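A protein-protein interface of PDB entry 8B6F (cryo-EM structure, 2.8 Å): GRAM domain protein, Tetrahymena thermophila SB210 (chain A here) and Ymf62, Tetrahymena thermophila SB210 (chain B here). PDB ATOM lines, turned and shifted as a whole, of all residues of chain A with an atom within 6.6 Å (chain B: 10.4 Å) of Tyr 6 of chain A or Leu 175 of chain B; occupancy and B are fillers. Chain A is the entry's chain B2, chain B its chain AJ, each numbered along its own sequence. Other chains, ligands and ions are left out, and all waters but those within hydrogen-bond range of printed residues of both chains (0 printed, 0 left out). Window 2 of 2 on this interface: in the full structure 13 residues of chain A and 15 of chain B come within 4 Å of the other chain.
Ser 4 of chain A touches none of the printed residues of chain B.
No residue of chain B comes within 4 Å of Gly 5 of chain A.
Tyr 6 of chain A touches just these residues of chain B: Leu 175 (3.7 Å) and Ile 180 (3.9 Å).
Printed residues of chain B within 4 Å of Asn 9 of chain A: Asn 164, Ile 166 and Thr 171.
Gly 10 of chain A touches two residues of chain B.
Gly 11 of chain A touches none of the printed residues of chain B.
No residue of chain B comes within 4 Å of Val 12 of chain A.
No residue of chain B comes within 4 Å of His 13 of chain A.
Of the printed residues of chain A, Asn 164 of chain B touches Asn 9 (3.6 Å).
Of the printed residues of chain A, Ile 166 of chain B touches Asn 9.
Of the printed residues of chain A, Pro 172 of chain B touches Leu 8 (2.9 Å).
Leu 175 of chain B touches just these residues of chain A: Tyr 6 and Gly 10.
Tyr 177 of chain B touches none of the printed residues of chain A.
Phe 185 of chain B touches none of the printed residues of chain A.
Hydrophobic or aromatic side chains of chain B that line the printed part of chain A: Ile 166, Pro 172, Leu 175 and Ile 180.
Among the printed residues, merely in contact across the chains: Tyr 6 of chain A with Leu 175 of chain B (3.7 Å), Tyr 6 of chain A with Ile 180 of chain B (3.9 Å), Leu 8 of chain A with Pro 172 of chain B (2.9 Å), Asn 9 of chain A with Asn 164 of chain B (3.6 Å), Asn 9 of chain A with Ile 166 of chain B (2.9 Å), Asn 9 of chain A with Thr 171 of chain B (3.9999 Å), Gly 10 of chain A with Thr 171 of chain B (3.5 Å) and Gly 10 of chain A with Leu 175 of chain B (3.7 Å).
The backbone NH of Ile 180 of chain B is in hydrogen-bond range of the backbone carbonyl oxygen of Leu 175 of chain B, 2.9 Å away.
OD1 of Asn 9 of chain A lies close to N of Gly 11 of chain A.
The side-chain amide oxygen of Asn 164 of chain B sits at hydrogen-bond distance from the backbone NH of Ile 166 of chain B, 2.7 Å away.
OG of Ser 7 of chain A is in hydrogen-bond range of OD1 of Asn 9 of chain A.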
ATOM      1  N   TYR A   3     -16.641 -28.258   3.460  1.00  0.00           N
ATOM      2  CA  TYR A   3     -17.397 -29.472   3.761  1.00  0.00           C
ATOM      3  C   TYR A   3     -18.806 -29.055   4.164  1.00  0.00           C
ATOM      4  O   TYR A   3     -19.064 -28.729   5.324  1.00  0.00           O
ATOM      5  CB  TYR A   3     -16.717 -30.276   4.862  1.00  0.00           C
ATOM      6  CG  TYR A   3     -17.452 -31.544   5.217  1.00  0.00           C
ATOM      7  CD1 TYR A   3     -17.251 -32.707   4.488  1.00  0.00           C
ATOM      8  CD2 TYR A   3     -18.348 -31.578   6.276  1.00  0.00           C
ATOM      9  CE1 TYR A   3     -17.918 -33.870   4.803  1.00  0.00           C
ATOM     10  CE2 TYR A   3     -19.023 -32.739   6.598  1.00  0.00           C
ATOM     11  CZ  TYR A   3     -18.804 -33.879   5.854  1.00  0.00           C
ATOM     12  OH  TYR A   3     -19.466 -35.037   6.164  1.00  0.00           O
ATOM     13  N   SER A   4     -19.723 -29.059   3.197  1.00  0.00           N
ATOM     14  CA  SER A   4     -21.091 -28.632   3.469  1.00  0.00           C
ATOM     15  C   SER A   4     -21.780 -29.562   4.459  1.00  0.00           C
ATOM     16  O   SER A   4     -22.537 -29.108   5.324  1.00  0.00           O
ATOM     17  CB  SER A   4     -21.880 -28.565   2.167  1.00  0.00           C
ATOM     18  OG  SER A   4     -21.938 -29.845   1.576  1.00  0.00           O
ATOM     19  N   GLY A   5     -21.538 -30.863   4.345  1.00  0.00           N
ATOM     20  CA  GLY A   5     -22.178 -31.832   5.209  1.00  0.00           C
ATOM     21  C   GLY A   5     -23.546 -32.293   4.761  1.00  0.00           C
ATOM     22  O   GLY A   5     -24.252 -32.928   5.552  1.00  0.00           O
ATOM     23  N   TYR A   6     -23.945 -31.997   3.529  1.00  0.00           N
ATOM     24  CA  TYR A   6     -25.221 -32.435   2.987  1.00  0.00           C
ATOM     25  C   TYR A   6     -25.033 -33.649   2.083  1.00  0.00           C
ATOM     26  O   TYR A   6     -23.943 -33.911   1.570  1.00  0.00           O
ATOM     27  CB  TYR A   6     -25.890 -31.311   2.196  1.00  0.00           C
ATOM     28  CG  TYR A   6     -26.328 -30.136   3.032  1.00  0.00           C
ATOM     29  CD1 TYR A   6     -27.508 -30.180   3.761  1.00  0.00           C
ATOM     30  CD2 TYR A   6     -25.573 -28.975   3.079  1.00  0.00           C
ATOM     31  CE1 TYR A   6     -27.917 -29.104   4.522  1.00  0.00           C
ATOM     32  CE2 TYR A   6     -25.972 -27.894   3.836  1.00  0.00           C
ATOM     33  CZ  TYR A   6     -27.144 -27.964   4.555  1.00  0.00           C
ATOM     34  OH  TYR A   6     -27.545 -26.888   5.309  1.00  0.00           O
ATOM     35  N   SER A   7     -26.120 -34.391   1.893  1.00  0.00           N
ATOM     36  CA  SER A   7     -26.133 -35.518   0.977  1.00  0.00           C
ATOM     37  C   SER A   7     -26.619 -35.042  -0.391  1.00  0.00           C
ATOM     38  O   SER A   7     -26.787 -33.844  -0.629  1.00  0.00           O
ATOM     39  CB  SER A   7     -26.997 -36.648   1.533  1.00  0.00           C
ATOM     40  OG  SER A   7     -28.351 -36.249   1.646  1.00  0.00           O
ATOM     41  N   LEU A   8     -26.849 -35.977  -1.309  1.00  0.00           N
ATOM     42  CA  LEU A   8     -27.310 -35.629  -2.646  1.00  0.00           C
ATOM     43  C   LEU A   8     -28.820 -35.455  -2.731  1.00  0.00           C
ATOM     44  O   LEU A   8     -29.326 -35.117  -3.806  1.00  0.00           O
ATOM     45  CB  LEU A   8     -26.861 -36.695  -3.650  1.00  0.00           C
ATOM     46  CG  LEU A   8     -25.349 -36.913  -3.781  1.00  0.00           C
ATOM     47  CD1 LEU A   8     -25.032 -37.830  -4.949  1.00  0.00           C
ATOM     48  CD2 LEU A   8     -24.593 -35.605  -3.892  1.00  0.00           C
ATOM     49  N   ASN A   9     -29.548 -35.681  -1.638  1.00  0.00           N
ATOM     50  CA  ASN A   9     -30.982 -35.424  -1.583  1.00  0.00           C
ATOM     51  C   ASN A   9     -31.326 -34.412  -0.497  1.00  0.00           C
ATOM     52  O   ASN A   9     -32.460 -34.390  -0.009  1.00  0.00           O
ATOM     53  CB  ASN A   9     -31.757 -36.723  -1.359  1.00  0.00           C
ATOM     54  CG  ASN A   9     -31.447 -37.363  -0.024  1.00  0.00           C
ATOM     55  OD1 ASN A   9     -30.369 -37.169   0.535  1.00  0.00           O
ATOM     56  ND2 ASN A   9     -32.393 -38.135   0.494  1.00  0.00           N
ATOM     57  N   GLY A  10     -30.367 -33.576  -0.106  1.00  0.00           N
ATOM     58  CA  GLY A  10     -30.574 -32.616   0.953  1.00  0.00           C
ATOM     59  C   GLY A  10     -30.400 -33.163   2.351  1.00  0.00           C
ATOM     60  O   GLY A  10     -30.537 -32.400   3.315  1.00  0.00           O
ATOM     61  N   GLY A  11     -30.099 -34.450   2.497  1.00  0.00           N
ATOM     62  CA  GLY A  11     -29.911 -35.056   3.801  1.00  0.00           C
ATOM     63  C   GLY A  11     -28.578 -34.688   4.411  1.00  0.00           C
ATOM     64  O   GLY A  11     -28.048 -33.592   4.197  1.00  0.00           O
ATOM     65  N   VAL A  12     -28.021 -35.616   5.184  1.00  0.00           N
ATOM     66  CA  VAL A  12     -26.756 -35.418   5.880  1.00  0.00           C
ATOM     67  C   VAL A  12     -25.694 -36.288   5.227  1.00  0.00           C
ATOM     68  O   VAL A  12     -25.932 -37.466   4.940  1.00  0.00           O
ATOM     69  CB  VAL A  12     -26.885 -35.723   7.383  1.00  0.00           C
ATOM     70  CG1 VAL A  12     -25.522 -35.961   8.020  1.00  0.00           C
ATOM     71  CG2 VAL A  12     -27.582 -34.575   8.078  1.00  0.00           C
ATOM     72  N   HIS A  13     -24.525 -35.700   4.997  1.00  0.00           N
ATOM     73  CA  HIS A  13     -23.430 -36.427   4.382  1.00  0.00           C
ATOM     74  C   HIS A  13     -23.038 -37.607   5.269  1.00  0.00           C
ATOM     75  O   HIS A  13     -22.949 -37.458   6.493  1.00  0.00           O
ATOM     76  CB  HIS A  13     -22.235 -35.494   4.179  1.00  0.00           C
ATOM     77  CG  HIS A  13     -21.208 -36.023   3.231  1.00  0.00           C
ATOM     78  ND1 HIS A  13     -20.031 -36.599   3.656  1.00  0.00           N
ATOM     79  CD2 HIS A  13     -21.176 -36.059   1.879  1.00  0.00           C
ATOM     80  CE1 HIS A  13     -19.320 -36.972   2.607  1.00  0.00           C
ATOM     81  NE2 HIS A  13     -19.992 -36.655   1.517  1.00  0.00           N
ATOM     82  N   PRO A  14     -22.799 -38.790   4.697  1.00  0.00           N
ATOM     83  CA  PRO A  14     -22.473 -39.951   5.539  1.00  0.00           C
ATOM     84  C   PRO A  14     -21.201 -39.786   6.352  1.00  0.00           C
ATOM     85  O   PRO A  14     -21.054 -40.460   7.378  1.00  0.00           O
ATOM     86  CB  PRO A  14     -22.347 -41.096   4.523  1.00  0.00           C
ATOM     87  CG  PRO A  14     -22.048 -40.428   3.233  1.00  0.00           C
ATOM     88  CD  PRO A  14     -22.791 -39.134   3.264  1.00  0.00           C
ATOM     89  N   ASN B 164     -39.043 -37.367   4.766  1.00  0.00           N
ATOM     90  CA  ASN B 164     -38.576 -36.578   3.636  1.00  0.00           C
ATOM     91  C   ASN B 164     -39.771 -36.047   2.854  1.00  0.00           C
ATOM     92  O   ASN B 164     -40.653 -36.815   2.458  1.00  0.00           O
ATOM     93  CB  ASN B 164     -37.683 -37.428   2.731  1.00  0.00           C
ATOM     94  CG  ASN B 164     -36.950 -36.604   1.695  1.00  0.00           C
ATOM     95  OD1 ASN B 164     -37.412 -35.539   1.291  1.00  0.00           O
ATOM     96  ND2 ASN B 164     -35.797 -37.096   1.258  1.00  0.00           N
ATOM     97  N   ILE B 166     -39.183 -33.776   0.144  1.00  0.00           N
ATOM     98  CA  ILE B 166     -38.690 -33.241  -1.117  1.00  0.00           C
ATOM     99  C   ILE B 166     -39.384 -33.932  -2.284  1.00  0.00           C
ATOM    100  O   ILE B 166     -39.723 -35.121  -2.224  1.00  0.00           O
ATOM    101  CB  ILE B 166     -37.160 -33.404  -1.198  1.00  0.00           C
ATOM    102  CG1 ILE B 166     -36.486 -32.609  -0.077  1.00  0.00           C
ATOM    103  CG2 ILE B 166     -36.637 -32.950  -2.556  1.00  0.00           C
ATOM    104  CD1 ILE B 166     -35.041 -32.983   0.150  1.00  0.00           C
ATOM    105  N   ASN B 168     -38.408 -32.621  -5.793  1.00  0.00           N
ATOM    106  CA  ASN B 168     -37.616 -32.300  -6.969  1.00  0.00           C
ATOM    107  C   ASN B 168     -36.153 -32.613  -6.693  1.00  0.00           C
ATOM    108  O   ASN B 168     -35.733 -32.763  -5.543  1.00  0.00           O
ATOM    109  CB  ASN B 168     -37.775 -30.828  -7.380  1.00  0.00           C
ATOM    110  CG  ASN B 168     -37.363 -29.868  -6.284  1.00  0.00           C
ATOM    111  OD1 ASN B 168     -36.190 -29.525  -6.150  1.00  0.00           O
ATOM    112  ND2 ASN B 168     -38.332 -29.420  -5.495  1.00  0.00           N
ATOM    113  N   ASP B 169     -35.379 -32.719  -7.772  1.00  0.00           N
ATOM    114  CA  ASP B 169     -33.960 -33.037  -7.693  1.00  0.00           C
ATOM    115  C   ASP B 169     -33.082 -31.792  -7.703  1.00  0.00           C
ATOM    116  O   ASP B 169     -31.893 -31.884  -8.024  1.00  0.00           O
ATOM    117  CB  ASP B 169     -33.566 -33.965  -8.842  1.00  0.00           C
ATOM    118  CG  ASP B 169     -34.280 -35.297  -8.781  1.00  0.00           C
ATOM    119  OD1 ASP B 169     -34.550 -35.777  -7.661  1.00  0.00           O
ATOM    120  OD2 ASP B 169     -34.571 -35.866  -9.853  1.00  0.00           O
ATOM    121  N   PHE B 170     -33.641 -30.633  -7.368  1.00  0.00           N
ATOM    122  CA  PHE B 170     -32.887 -29.391  -7.281  1.00  0.00           C
ATOM    123  C   PHE B 170     -32.457 -29.066  -5.857  1.00  0.00           C
ATOM    124  O   PHE B 170     -31.889 -27.995  -5.624  1.00  0.00           O
ATOM    125  CB  PHE B 170     -33.707 -28.229  -7.845  1.00  0.00           C
ATOM    126  CG  PHE B 170     -33.867 -28.265  -9.335  1.00  0.00           C
ATOM    127  CD1 PHE B 170     -34.928 -28.937  -9.916  1.00  0.00           C
ATOM    128  CD2 PHE B 170     -32.963 -27.611 -10.155  1.00  0.00           C
ATOM    129  CE1 PHE B 170     -35.078 -28.966 -11.288  1.00  0.00           C
ATOM    130  CE2 PHE B 170     -33.107 -27.637 -11.527  1.00  0.00           C
ATOM    131  CZ  PHE B 170     -34.167 -28.313 -12.095  1.00  0.00           C
ATOM    132  N   THR B 171     -32.707 -29.961  -4.904  1.00  0.00           N
ATOM    133  CA  THR B 171     -32.389 -29.658  -3.510  1.00  0.00           C
ATOM    134  C   THR B 171     -30.900 -29.435  -3.292  1.00  0.00           C
ATOM    135  O   THR B 171     -30.536 -28.439  -2.646  1.00  0.00           O
ATOM    136  CB  THR B 171     -32.934 -30.763  -2.601  1.00  0.00           C
ATOM    137  OG1 THR B 171     -34.365 -30.750  -2.639  1.00  0.00           O
ATOM    138  CG2 THR B 171     -32.475 -30.559  -1.159  1.00  0.00           C
ATOM    139  N   PRO B 172     -29.997 -30.299  -3.763  1.00  0.00           N
ATOM    140  CA  PRO B 172     -28.569 -29.973  -3.622  1.00  0.00           C
ATOM    141  C   PRO B 172     -28.189 -28.680  -4.315  1.00  0.00           C
ATOM    142  O   PRO B 172     -27.354 -27.925  -3.804  1.00  0.00           O
ATOM    143  CB  PRO B 172     -27.868 -31.187  -4.250  1.00  0.00           C
ATOM    144  CG  PRO B 172     -28.875 -32.272  -4.223  1.00  0.00           C
ATOM    145  CD  PRO B 172     -30.194 -31.602  -4.419  1.00  0.00           C
ATOM    146  N   LEU B 173     -28.778 -28.406  -5.479  1.00  0.00           N
ATOM    147  CA  LEU B 173     -28.433 -27.192  -6.209  1.00  0.00           C
ATOM    148  C   LEU B 173     -28.829 -25.944  -5.429  1.00  0.00           C
ATOM    149  O   LEU B 173     -28.067 -24.973  -5.375  1.00  0.00           O
ATOM    150  CB  LEU B 173     -29.103 -27.213  -7.583  1.00  0.00           C
ATOM    151  CG  LEU B 173     -28.634 -28.336  -8.515  1.00  0.00           C
ATOM    152  CD1 LEU B 173     -29.446 -28.343  -9.798  1.00  0.00           C
ATOM    153  CD2 LEU B 173     -27.150 -28.213  -8.830  1.00  0.00           C
ATOM    154  N   THR B 174     -30.018 -25.946  -4.821  1.00  0.00           N
ATOM    155  CA  THR B 174     -30.433 -24.792  -4.026  1.00  0.00           C
ATOM    156  C   THR B 174     -29.621 -24.683  -2.742  1.00  0.00           C
ATOM    157  O   THR B 174     -29.234 -23.580  -2.339  1.00  0.00           O
ATOM    158  CB  THR B 174     -31.931 -24.859  -3.718  1.00  0.00           C
ATOM    159  OG1 THR B 174     -32.312 -23.719  -2.937  1.00  0.00           O
ATOM    160  CG2 THR B 174     -32.285 -26.116  -2.957  1.00  0.00           C
ATOM    161  N   LEU B 175     -29.359 -25.811  -2.080  1.00  0.00           N
ATOM    162  CA  LEU B 175     -28.540 -25.780  -0.873  1.00  0.00           C
ATOM    163  C   LEU B 175     -27.134 -25.281  -1.158  1.00  0.00           C
ATOM    164  O   LEU B 175     -26.463 -24.768  -0.257  1.00  0.00           O
ATOM    165  CB  LEU B 175     -28.478 -27.171  -0.247  1.00  0.00           C
ATOM    166  CG  LEU B 175     -29.650 -27.555   0.649  1.00  0.00           C
ATOM    167  CD1 LEU B 175     -29.657 -29.044   0.917  1.00  0.00           C
ATOM    168  CD2 LEU B 175     -29.546 -26.780   1.948  1.00  0.00           C
ATOM    169  N   SER B 176     -26.664 -25.435  -2.391  1.00  0.00           N
ATOM    170  CA  SER B 176     -25.347 -24.942  -2.761  1.00  0.00           C
ATOM    171  C   SER B 176     -25.357 -23.482  -3.198  1.00  0.00           C
ATOM    172  O   SER B 176     -24.594 -22.667  -2.671  1.00  0.00           O
ATOM    173  CB  SER B 176     -24.768 -25.794  -3.881  1.00  0.00           C
ATOM    174  OG  SER B 176     -23.466 -25.340  -4.156  1.00  0.00           O
ATOM    175  N   TYR B 177     -26.219 -23.137  -4.152  1.00  0.00           N
ATOM    176  CA  TYR B 177     -26.186 -21.808  -4.745  1.00  0.00           C
ATOM    177  C   TYR B 177     -26.769 -20.752  -3.821  1.00  0.00           C
ATOM    178  O   TYR B 177     -26.346 -19.592  -3.875  1.00  0.00           O
ATOM    179  CB  TYR B 177     -26.936 -21.803  -6.079  1.00  0.00           C
ATOM    180  CG  TYR B 177     -26.381 -22.767  -7.099  1.00  0.00           C
ATOM    181  CD1 TYR B 177     -25.013 -22.879  -7.304  1.00  0.00           C
ATOM    182  CD2 TYR B 177     -27.224 -23.572  -7.853  1.00  0.00           C
ATOM    183  CE1 TYR B 177     -24.499 -23.759  -8.233  1.00  0.00           C
ATOM    184  CE2 TYR B 177     -26.719 -24.454  -8.786  1.00  0.00           C
ATOM    185  CZ  TYR B 177     -25.356 -24.543  -8.972  1.00  0.00           C
ATOM    186  OH  TYR B 177     -24.848 -25.425  -9.895  1.00  0.00           O
ATOM    187  N   TYR B 178     -27.733 -21.117  -2.980  1.00  0.00           N
ATOM    188  CA  TYR B 178     -28.458 -20.140  -2.186  1.00  0.00           C
ATOM    189  C   TYR B 178     -28.224 -20.272  -0.690  1.00  0.00           C
ATOM    190  O   TYR B 178     -28.635 -19.380   0.058  1.00  0.00           O
ATOM    191  CB  TYR B 178     -29.962 -20.247  -2.479  1.00  0.00           C
ATOM    192  CG  TYR B 178     -30.297 -19.921  -3.914  1.00  0.00           C
ATOM    193  CD1 TYR B 178     -30.160 -20.876  -4.912  1.00  0.00           C
ATOM    194  CD2 TYR B 178     -30.733 -18.655  -4.274  1.00  0.00           C
ATOM    195  CE1 TYR B 178     -30.453 -20.583  -6.226  1.00  0.00           C
ATOM    196  CE2 TYR B 178     -31.029 -18.350  -5.587  1.00  0.00           C
ATOM    197  CZ  TYR B 178     -30.886 -19.318  -6.559  1.00  0.00           C
ATOM    198  OH  TYR B 178     -31.181 -19.024  -7.868  1.00  0.00           O
ATOM    199  N   SER B 179     -27.586 -21.349  -0.228  1.00  0.00           N
ATOM    200  CA  SER B 179     -27.279 -21.496   1.191  1.00  0.00           C
ATOM    201  C   SER B 179     -25.779 -21.533   1.454  1.00  0.00           C
ATOM    202  O   SER B 179     -25.282 -20.718   2.237  1.00  0.00           O
ATOM    203  CB  SER B 179     -27.956 -22.758   1.743  1.00  0.00           C
ATOM    204  OG  SER B 179     -27.737 -22.882   3.137  1.00  0.00           O
ATOM    205  N   ILE B 180     -25.035 -22.436   0.815  1.00  0.00           N
ATOM    206  CA  ILE B 180     -23.634 -22.660   1.165  1.00  0.00           C
ATOM    207  C   ILE B 180     -22.717 -21.842   0.267  1.00  0.00           C
ATOM    208  O   ILE B 180     -21.914 -21.038   0.753  1.00  0.00           O
ATOM    209  CB  ILE B 180     -23.279 -24.158   1.083  1.00  0.00           C
ATOM    210  CG1 ILE B 180     -24.145 -24.973   2.050  1.00  0.00           C
ATOM    211  CG2 ILE B 180     -21.797 -24.379   1.375  1.00  0.00           C
ATOM    212  CD1 ILE B 180     -23.970 -24.609   3.515  1.00  0.00           C
ATOM    213  N   ASN B 181     -22.823 -22.043  -1.048  1.00  0.00           N
ATOM    214  CA  ASN B 181     -21.977 -21.353  -2.015  1.00  0.00           C
ATOM    215  C   ASN B 181     -22.614 -20.075  -2.534  1.00  0.00           C
ATOM    216  O   ASN B 181     -22.342 -19.664  -3.669  1.00  0.00           O
ATOM    217  CB  ASN B 181     -21.635 -22.286  -3.177  1.00  0.00           C
ATOM    218  CG  ASN B 181     -20.987 -23.575  -2.716  1.00  0.00           C
ATOM    219  OD1 ASN B 181     -21.659 -24.584  -2.505  1.00  0.00           O
ATOM    220  ND2 ASN B 181     -19.671 -23.546  -2.557  1.00  0.00           N
ATOM    221  N   SER B 182     -23.452 -19.433  -1.724  1.00  0.00           N
ATOM    222  CA  SER B 182     -24.082 -18.186  -2.139  1.00  0.00           C
ATOM    223  C   SER B 182     -23.049 -17.109  -2.437  1.00  0.00           C
ATOM    224  O   SER B 182     -23.293 -16.234  -3.273  1.00  0.00           O
ATOM    225  CB  SER B 182     -25.060 -17.726  -1.063  1.00  0.00           C
ATOM    226  OG  SER B 182     -24.478 -17.819   0.222  1.00  0.00           O
ATOM    227  N   ALA B 183     -21.893 -17.157  -1.775  1.00  0.00           N
ATOM    228  CA  ALA B 183     -20.830 -16.210  -2.094  1.00  0.00           C
ATOM    229  C   ALA B 183     -20.397 -16.359  -3.545  1.00  0.00           C
ATOM    230  O   ALA B 183     -20.258 -15.367  -4.270  1.00  0.00           O
ATOM    231  CB  ALA B 183     -19.644 -16.416  -1.152  1.00  0.00           C
ATOM    232  N   GLU B 184     -20.180 -17.598  -3.990  1.00  0.00           N
ATOM    233  CA  GLU B 184     -19.807 -17.828  -5.381  1.00  0.00           C
ATOM    234  C   GLU B 184     -20.966 -17.529  -6.322  1.00  0.00           C
ATOM    235  O   GLU B 184     -20.744 -17.122  -7.467  1.00  0.00           O
ATOM    236  CB  GLU B 184     -19.326 -19.265  -5.572  1.00  0.00           C
ATOM    237  CG  GLU B 184     -17.945 -19.532  -4.994  1.00  0.00           C
ATOM    238  CD  GLU B 184     -17.917 -19.464  -3.482  1.00  0.00           C
ATOM    239  OE1 GLU B 184     -18.990 -19.270  -2.875  1.00  0.00           O
ATOM    240  OE2 GLU B 184     -16.822 -19.601  -2.900  1.00  0.00           O
ATOM    241  N   PHE B 185     -22.201 -17.729  -5.861  1.00  0.00           N
ATOM    242  CA  PHE B 185     -23.362 -17.350  -6.658  1.00  0.00           C
ATOM    243  C   PHE B 185     -23.358 -15.851  -6.937  1.00  0.00           C
ATOM    244  O   PHE B 185     -23.556 -15.419  -8.077  1.00  0.00           O
ATOM    245  CB  PHE B 185     -24.638 -17.770  -5.926  1.00  0.00           C
ATOM    246  CG  PHE B 185     -25.900 -17.499  -6.689  1.00  0.00           C
ATOM    247  CD1 PHE B 185     -26.255 -18.287  -7.770  1.00  0.00           C
ATOM    248  CD2 PHE B 185     -26.753 -16.478  -6.301  1.00  0.00           C
ATOM    249  CE1 PHE B 185     -27.423 -18.046  -8.466  1.00  0.00           C
ATOM    250  CE2 PHE B 185     -27.921 -16.233  -6.992  1.00  0.00           C
ATOM    251  CZ  PHE B 185     -28.258 -17.020  -8.076  1.00  0.00           C
